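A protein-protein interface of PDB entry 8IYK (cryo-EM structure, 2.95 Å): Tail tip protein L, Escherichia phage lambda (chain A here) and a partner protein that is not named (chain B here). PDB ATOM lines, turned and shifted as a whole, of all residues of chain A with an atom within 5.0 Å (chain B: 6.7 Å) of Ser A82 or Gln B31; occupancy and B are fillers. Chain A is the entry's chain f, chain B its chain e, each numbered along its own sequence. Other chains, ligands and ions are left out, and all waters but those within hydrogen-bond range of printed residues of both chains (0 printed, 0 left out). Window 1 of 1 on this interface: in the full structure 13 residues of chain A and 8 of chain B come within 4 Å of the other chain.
The side-chain amide oxygen of Gln B31 sits at hydrogen-bond distance from the side-chain hydroxyl of Ser A82, 2.9 Å away.
The backbone carbonyl oxygen of Arg B32 lies within hydrogen-bond range of the side-chain hydroxyl of Tyr A85 (3.4 Å).
The backbone carbonyl oxygen of Arg B21 sits at hydrogen-bond distance from the backbone NH of Ala B33 (2.9 Å).
O of Val B23 lies within hydrogen-bond range of N of Gln B31 (2.9 Å).
The side-chain hydroxyl of Tyr A59 sits at hydrogen-bond distance from the backbone carbonyl oxygen of Ser A82 (2.5 Å).
The backbone carbonyl oxygen (O) of Pro A60 is in hydrogen-bond range of the backbone NH (N) of Ser A82, at 3.1 Å.
The side-chain hydroxyl (OG) of Ser A82 is in hydrogen-bond range of the backbone NH (N) of Leu A84.
The backbone NH (N) of Asn A83 is in hydrogen-bond range of the backbone carbonyl oxygen (O) of Val A146 (2.8 Å).
Among the printed residues, merely in contact across the chains: Leu A84 with Arg B21 (3.4 Å), Leu A84 with Gln B31 (3.5 Å), Ser A82 with Val B23 (3.5 Å), Leu A84 with Val B23 (3.6 Å), Pro A60 with Phe B25 (3.7 Å), Thr A80 with Phe B25 (3.7 Å), Val A146 with Val B23 (3.7 Å), Tyr A85 with Gln B31 (3.8 Å), Leu A84 with Ala B33 (3.8 Å), Tyr A59 with Gln B31 (3.8 Å), Pro A60 with Tyr B29 (3.8 Å), Val A146 with Arg B21 (3.9 Å), Tyr A59 with Tyr B29 (3.9 Å) and Leu A84 with Arg B32 (3.98 Å).
Printed residues of chain A that touch a printed residue of chain B: Tyr A59, Pro A60, Thr A80, Ser A82, Leu A84, Tyr A85 and Val A146.
Hydrophobic or aromatic side chains of chain B that line the printed part of chain A: Val B23, Phe B25, Tyr B29 and Ala B33.
Among the printed residues, no Asp or Glu carboxylate lies within 4 Å of a Lys or Arg side-chain nitrogen of the other chain.
Of the printed residues of chain A, Gln B31 touches Tyr A59 (3.8 Å), Ser A82 (2.9 Å), Leu A84 (3.5 Å) and Tyr A85 (3.8 Å).
Of the printed residues of chain A, Phe B25 touches Pro A60 and Thr A80.
Of the printed residues of chain A, Val B23 touches Ser A82 (3.5 Å), Leu A84 (3.6 Å) and Val A146 (3.7 Å).
The nearest residue of chain B that does not touch Ser A82 is Phe B25 (4.5 Å).
The nearest printed residue of chain A that does not touch Gln B31 is Pro A60 (4.02 Å).
The nearest printed residue of chain A that does not touch Tyr B29 is Tyr A85 (7.4 Å).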
ATOM      1  N   TYR A  59      -4.589  13.627  -4.449  1.00  0.00           N
ATOM      2  CA  TYR A  59      -4.997  12.291  -4.042  1.00  0.00           C
ATOM      3  C   TYR A  59      -5.076  12.239  -2.522  1.00  0.00           C
ATOM      4  O   TYR A  59      -4.181  12.752  -1.841  1.00  0.00           O
ATOM      5  CB  TYR A  59      -4.014  11.245  -4.570  1.00  0.00           C
ATOM      6  CG  TYR A  59      -4.614   9.872  -4.752  1.00  0.00           C
ATOM      7  CD1 TYR A  59      -5.576   9.635  -5.724  1.00  0.00           C
ATOM      8  CD2 TYR A  59      -4.212   8.810  -3.958  1.00  0.00           C
ATOM      9  CE1 TYR A  59      -6.124   8.380  -5.893  1.00  0.00           C
ATOM     10  CE2 TYR A  59      -4.754   7.554  -4.120  1.00  0.00           C
ATOM     11  CZ  TYR A  59      -5.710   7.344  -5.088  1.00  0.00           C
ATOM     12  OH  TYR A  59      -6.250   6.090  -5.252  1.00  0.00           O
ATOM     13  N   PRO A  60      -6.127  11.648  -1.953  1.00  0.00           N
ATOM     14  CA  PRO A  60      -6.219  11.565  -0.490  1.00  0.00           C
ATOM     15  C   PRO A  60      -5.110  10.715   0.108  1.00  0.00           C
ATOM     16  O   PRO A  60      -5.082   9.496  -0.078  1.00  0.00           O
ATOM     17  CB  PRO A  60      -7.599  10.938  -0.255  1.00  0.00           C
ATOM     18  CG  PRO A  60      -8.342  11.130  -1.538  1.00  0.00           C
ATOM     19  CD  PRO A  60      -7.315  11.090  -2.617  1.00  0.00           C
ATOM     20  N   THR A  80      -1.612   6.158   4.918  1.00  0.00           N
ATOM     21  CA  THR A  80      -2.931   5.760   4.453  1.00  0.00           C
ATOM     22  C   THR A  80      -3.263   6.524   3.181  1.00  0.00           C
ATOM     23  O   THR A  80      -3.084   7.744   3.117  1.00  0.00           O
ATOM     24  CB  THR A  80      -3.994   6.027   5.518  1.00  0.00           C
ATOM     25  OG1 THR A  80      -3.405   5.920   6.820  1.00  0.00           O
ATOM     26  CG2 THR A  80      -5.130   5.028   5.396  1.00  0.00           C
ATOM     27  N   VAL A  81      -3.743   5.804   2.172  1.00  0.00           N
ATOM     28  CA  VAL A  81      -4.018   6.381   0.865  1.00  0.00           C
ATOM     29  C   VAL A  81      -5.351   5.842   0.364  1.00  0.00           C
ATOM     30  O   VAL A  81      -5.825   4.791   0.806  1.00  0.00           O
ATOM     31  CB  VAL A  81      -2.873   6.079  -0.127  1.00  0.00           C
ATOM     32  CG1 VAL A  81      -3.042   4.704  -0.727  1.00  0.00           C
ATOM     33  CG2 VAL A  81      -2.796   7.144  -1.206  1.00  0.00           C
ATOM     34  N   SER A  82      -5.970   6.584  -0.549  1.00  0.00           N
ATOM     35  CA  SER A  82      -7.270   6.196  -1.074  1.00  0.00           C
ATOM     36  C   SER A  82      -7.129   5.074  -2.094  1.00  0.00           C
ATOM     37  O   SER A  82      -6.276   5.125  -2.982  1.00  0.00           O
ATOM     38  CB  SER A  82      -7.959   7.395  -1.718  1.00  0.00           C
ATOM     39  OG  SER A  82      -9.186   7.016  -2.314  1.00  0.00           O
ATOM     40  N   ASN A  83      -7.978   4.055  -1.968  1.00  0.00           N
ATOM     41  CA  ASN A  83      -8.023   2.967  -2.934  1.00  0.00           C
ATOM     42  C   ASN A  83      -9.313   2.972  -3.745  1.00  0.00           C
ATOM     43  O   ASN A  83      -9.680   1.949  -4.333  1.00  0.00           O
ATOM     44  CB  ASN A  83      -7.838   1.618  -2.240  1.00  0.00           C
ATOM     45  CG  ASN A  83      -7.524   0.502  -3.215  1.00  0.00           C
ATOM     46  OD1 ASN A  83      -6.684   0.656  -4.098  1.00  0.00           O
ATOM     47  ND2 ASN A  83      -8.222  -0.616  -3.080  1.00  0.00           N
ATOM     48  N   LEU A  84     -10.019   4.096  -3.782  1.00  0.00           N
ATOM     49  CA  LEU A  84     -11.136   4.215  -4.705  1.00  0.00           C
ATOM     50  C   LEU A  84     -10.625   4.140  -6.139  1.00  0.00           C
ATOM     51  O   LEU A  84      -9.515   4.582  -6.449  1.00  0.00           O
ATOM     52  CB  LEU A  84     -11.892   5.522  -4.476  1.00  0.00           C
ATOM     53  CG  LEU A  84     -12.857   5.548  -3.291  1.00  0.00           C
ATOM     54  CD1 LEU A  84     -13.728   6.787  -3.346  1.00  0.00           C
ATOM     55  CD2 LEU A  84     -13.712   4.297  -3.272  1.00  0.00           C
ATOM     56  N   TYR A  85     -11.442   3.551  -7.010  1.00  0.00           N
ATOM     57  CA  TYR A  85     -11.146   3.320  -8.421  1.00  0.00           C
ATOM     58  C   TYR A  85     -10.026   2.309  -8.629  1.00  0.00           C
ATOM     59  O   TYR A  85      -9.480   2.223  -9.736  1.00  0.00           O
ATOM     60  CB  TYR A  85     -10.810   4.627  -9.150  1.00  0.00           C
ATOM     61  CG  TYR A  85     -11.747   5.758  -8.796  1.00  0.00           C
ATOM     62  CD1 TYR A  85     -13.122   5.582  -8.837  1.00  0.00           C
ATOM     63  CD2 TYR A  85     -11.256   6.996  -8.409  1.00  0.00           C
ATOM     64  CE1 TYR A  85     -13.983   6.608  -8.508  1.00  0.00           C
ATOM     65  CE2 TYR A  85     -12.110   8.029  -8.079  1.00  0.00           C
ATOM     66  CZ  TYR A  85     -13.472   7.829  -8.131  1.00  0.00           C
ATOM     67  OH  TYR A  85     -14.330   8.854  -7.803  1.00  0.00           O
ATOM     68  N   VAL A  88      -4.373   1.842  -6.238  1.00  0.00           N
ATOM     69  CA  VAL A  88      -3.335   1.167  -5.461  1.00  0.00           C
ATOM     70  C   VAL A  88      -3.389  -0.336  -5.693  1.00  0.00           C
ATOM     71  O   VAL A  88      -2.354  -1.011  -5.733  1.00  0.00           O
ATOM     72  CB  VAL A  88      -3.477   1.518  -3.971  1.00  0.00           C
ATOM     73  CG1 VAL A  88      -2.456   0.761  -3.144  1.00  0.00           C
ATOM     74  CG2 VAL A  88      -3.323   3.007  -3.782  1.00  0.00           C
ATOM     75  N   VAL A 146     -11.902   0.565  -0.260  1.00  0.00           N
ATOM     76  CA  VAL A 146     -11.936   1.973   0.130  1.00  0.00           C
ATOM     77  C   VAL A 146     -10.533   2.564   0.197  1.00  0.00           C
ATOM     78  O   VAL A 146     -10.238   3.562  -0.462  1.00  0.00           O
ATOM     79  CB  VAL A 146     -12.687   2.162   1.467  1.00  0.00           C
ATOM     80  CG1 VAL A 146     -13.109   3.607   1.633  1.00  0.00           C
ATOM     81  CG2 VAL A 146     -13.894   1.247   1.529  1.00  0.00           C
ATOM     82  N   SER A 147      -9.647   1.959   0.989  1.00  0.00           N
ATOM     83  CA  SER A 147      -8.332   2.547   1.209  1.00  0.00           C
ATOM     84  C   SER A 147      -7.207   1.523   1.192  1.00  0.00           C
ATOM     85  O   SER A 147      -7.424   0.343   0.903  1.00  0.00           O
ATOM     86  CB  SER A 147      -8.307   3.291   2.541  1.00  0.00           C
ATOM     87  OG  SER A 147      -7.781   2.469   3.567  1.00  0.00           O
ATOM     88  N   ALA A 148      -5.997   1.983   1.506  1.00  0.00           N
ATOM     89  CA  ALA A 148      -4.833   1.114   1.608  1.00  0.00           C
ATOM     90  C   ALA A 148      -3.852   1.735   2.588  1.00  0.00           C
ATOM     91  O   ALA A 148      -3.528   2.920   2.473  1.00  0.00           O
ATOM     92  CB  ALA A 148      -4.174   0.908   0.243  1.00  0.00           C
ATOM     93  N   ARG B  21     -19.333   5.371  -0.567  1.00  0.00           N
ATOM     94  CA  ARG B  21     -17.967   5.214  -0.085  1.00  0.00           C
ATOM     95  C   ARG B  21     -17.274   6.568  -0.149  1.00  0.00           C
ATOM     96  O   ARG B  21     -17.135   7.146  -1.230  1.00  0.00           O
ATOM     97  CB  ARG B  21     -17.206   4.177  -0.911  1.00  0.00           C
ATOM     98  CG  ARG B  21     -17.696   2.754  -0.728  1.00  0.00           C
ATOM     99  CD  ARG B  21     -16.637   1.748  -1.140  1.00  0.00           C
ATOM    100  NE  ARG B  21     -17.123   0.821  -2.155  1.00  0.00           N
ATOM    101  CZ  ARG B  21     -16.832   0.904  -3.445  1.00  0.00           C
ATOM    102  NH1 ARG B  21     -16.058   1.866  -3.918  1.00  0.00           N
ATOM    103  NH2 ARG B  21     -17.332   0.000  -4.281  1.00  0.00           N
ATOM    104  N   LYS B  22     -16.844   7.068   1.005  1.00  0.00           N
ATOM    105  CA  LYS B  22     -16.235   8.385   1.121  1.00  0.00           C
ATOM    106  C   LYS B  22     -14.790   8.238   1.569  1.00  0.00           C
ATOM    107  O   LYS B  22     -14.510   7.530   2.541  1.00  0.00           O
ATOM    108  CB  LYS B  22     -17.004   9.256   2.118  1.00  0.00           C
ATOM    109  CG  LYS B  22     -17.910  10.291   1.485  1.00  0.00           C
ATOM    110  CD  LYS B  22     -17.120  11.519   1.072  1.00  0.00           C
ATOM    111  CE  LYS B  22     -16.663  12.314   2.281  1.00  0.00           C
ATOM    112  NZ  LYS B  22     -16.687  13.780   2.018  1.00  0.00           N
ATOM    113  N   VAL B  23     -13.878   8.904   0.864  1.00  0.00           N
ATOM    114  CA  VAL B  23     -12.481   8.980   1.271  1.00  0.00           C
ATOM    115  C   VAL B  23     -12.088  10.447   1.323  1.00  0.00           C
ATOM    116  O   VAL B  23     -12.087  11.130   0.292  1.00  0.00           O
ATOM    117  CB  VAL B  23     -11.550   8.207   0.325  1.00  0.00           C
ATOM    118  CG1 VAL B  23     -10.176   8.081   0.944  1.00  0.00           C
ATOM    119  CG2 VAL B  23     -12.121   6.834   0.025  1.00  0.00           C
ATOM    120  N   ARG B  24     -11.747  10.927   2.516  1.00  0.00           N
ATOM    121  CA  ARG B  24     -11.330  12.315   2.693  1.00  0.00           C
ATOM    122  C   ARG B  24     -10.545  12.410   3.988  1.00  0.00           C
ATOM    123  O   ARG B  24     -11.100  12.172   5.064  1.00  0.00           O
ATOM    124  CB  ARG B  24     -12.536  13.251   2.720  1.00  0.00           C
ATOM    125  CG  ARG B  24     -12.191  14.707   2.974  1.00  0.00           C
ATOM    126  CD  ARG B  24     -13.349  15.610   2.589  1.00  0.00           C
ATOM    127  NE  ARG B  24     -13.499  16.744   3.491  1.00  0.00           N
ATOM    128  CZ  ARG B  24     -13.571  18.008   3.095  1.00  0.00           C
ATOM    129  NH1 ARG B  24     -13.505  18.336   1.816  1.00  0.00           N
ATOM    130  NH2 ARG B  24     -13.713  18.965   4.007  1.00  0.00           N
ATOM    131  N   PHE B  25      -9.266  12.754   3.887  1.00  0.00           N
ATOM    132  CA  PHE B  25      -8.395  12.885   5.045  1.00  0.00           C
ATOM    133  C   PHE B  25      -8.311  14.357   5.421  1.00  0.00           C
ATOM    134  O   PHE B  25      -7.884  15.184   4.610  1.00  0.00           O
ATOM    135  CB  PHE B  25      -7.007  12.324   4.744  1.00  0.00           C
ATOM    136  CG  PHE B  25      -6.982  10.835   4.571  1.00  0.00           C
ATOM    137  CD1 PHE B  25      -7.185  10.269   3.326  1.00  0.00           C
ATOM    138  CD2 PHE B  25      -6.757  10.001   5.648  1.00  0.00           C
ATOM    139  CE1 PHE B  25      -7.166   8.900   3.161  1.00  0.00           C
ATOM    140  CE2 PHE B  25      -6.735   8.633   5.485  1.00  0.00           C
ATOM    141  CZ  PHE B  25      -6.940   8.082   4.241  1.00  0.00           C
ATOM    142  N   TYR B  29      -8.377  16.747  -0.440  1.00  0.00           N
ATOM    143  CA  TYR B  29      -9.102  16.158  -1.558  1.00  0.00           C
ATOM    144  C   TYR B  29     -10.086  15.106  -1.065  1.00  0.00           C
ATOM    145  O   TYR B  29      -9.819  14.381  -0.103  1.00  0.00           O
ATOM    146  CB  TYR B  29      -8.122  15.532  -2.548  1.00  0.00           C
ATOM    147  CG  TYR B  29      -8.630  15.493  -3.967  1.00  0.00           C
ATOM    148  CD1 TYR B  29      -8.374  14.403  -4.785  1.00  0.00           C
ATOM    149  CD2 TYR B  29      -9.352  16.552  -4.493  1.00  0.00           C
ATOM    150  CE1 TYR B  29      -8.836  14.362  -6.085  1.00  0.00           C
ATOM    151  CE2 TYR B  29      -9.814  16.522  -5.792  1.00  0.00           C
ATOM    152  CZ  TYR B  29      -9.554  15.426  -6.583  1.00  0.00           C
ATOM    153  OH  TYR B  29     -10.014  15.391  -7.878  1.00  0.00           O
ATOM    154  N   SER B  30     -11.234  15.023  -1.735  1.00  0.00           N
ATOM    155  CA  SER B  30     -12.288  14.087  -1.376  1.00  0.00           C
ATOM    156  C   SER B  30     -12.672  13.256  -2.588  1.00  0.00           C
ATOM    157  O   SER B  30     -12.741  13.770  -3.707  1.00  0.00           O
ATOM    158  CB  SER B  30     -13.523  14.813  -0.843  1.00  0.00           C
ATOM    159  OG  SER B  30     -14.519  14.919  -1.845  1.00  0.00           O
ATOM    160  N   GLN B  31     -12.923  11.969  -2.359  1.00  0.00           N
ATOM    161  CA  GLN B  31     -13.362  11.062  -3.410  1.00  0.00           C
ATOM    162  C   GLN B  31     -14.600  10.314  -2.940  1.00  0.00           C
ATOM    163  O   GLN B  31     -14.636   9.802  -1.816  1.00  0.00           O
ATOM    164  CB  GLN B  31     -12.253  10.082  -3.797  1.00  0.00           C
ATOM    165  CG  GLN B  31     -11.094  10.732  -4.526  1.00  0.00           C
ATOM    166  CD  GLN B  31     -10.140   9.720  -5.122  1.00  0.00           C
ATOM    167  OE1 GLN B  31      -9.945   8.636  -4.573  1.00  0.00           O
ATOM    168  NE2 GLN B  31      -9.538  10.069  -6.251  1.00  0.00           N
ATOM    169  N   ARG B  32     -15.611  10.259  -3.800  1.00  0.00           N
ATOM    170  CA  ARG B  32     -16.889   9.640  -3.485  1.00  0.00           C
ATOM    171  C   ARG B  32     -17.223   8.577  -4.521  1.00  0.00           C
ATOM    172  O   ARG B  32     -17.062   8.796  -5.726  1.00  0.00           O
ATOM    173  CB  ARG B  32     -18.005  10.684  -3.430  1.00  0.00           C
ATOM    174  CG  ARG B  32     -17.817  11.737  -2.359  1.00  0.00           C
ATOM    175  CD  ARG B  32     -18.592  13.002  -2.673  1.00  0.00           C
ATOM    176  NE  ARG B  32     -17.714  14.092  -3.079  1.00  0.00           N
ATOM    177  CZ  ARG B  32     -17.474  14.436  -4.336  1.00  0.00           C
ATOM    178  NH1 ARG B  32     -18.040  13.798  -5.347  1.00  0.00           N
ATOM    179  NH2 ARG B  32     -16.647  15.446  -4.586  1.00  0.00           N
ATOM    180  N   ALA B  33     -17.694   7.431  -4.045  1.00  0.00           N
ATOM    181  CA  ALA B  33     -18.071   6.311  -4.889  1.00  0.00           C
ATOM    182  C   ALA B  33     -19.468   5.836  -4.517  1.00  0.00           C
ATOM    183  O   ALA B  33     -19.883   5.965  -3.362  1.00  0.00           O
ATOM    184  CB  ALA B  33     -17.075   5.152  -4.750  1.00  0.00           C
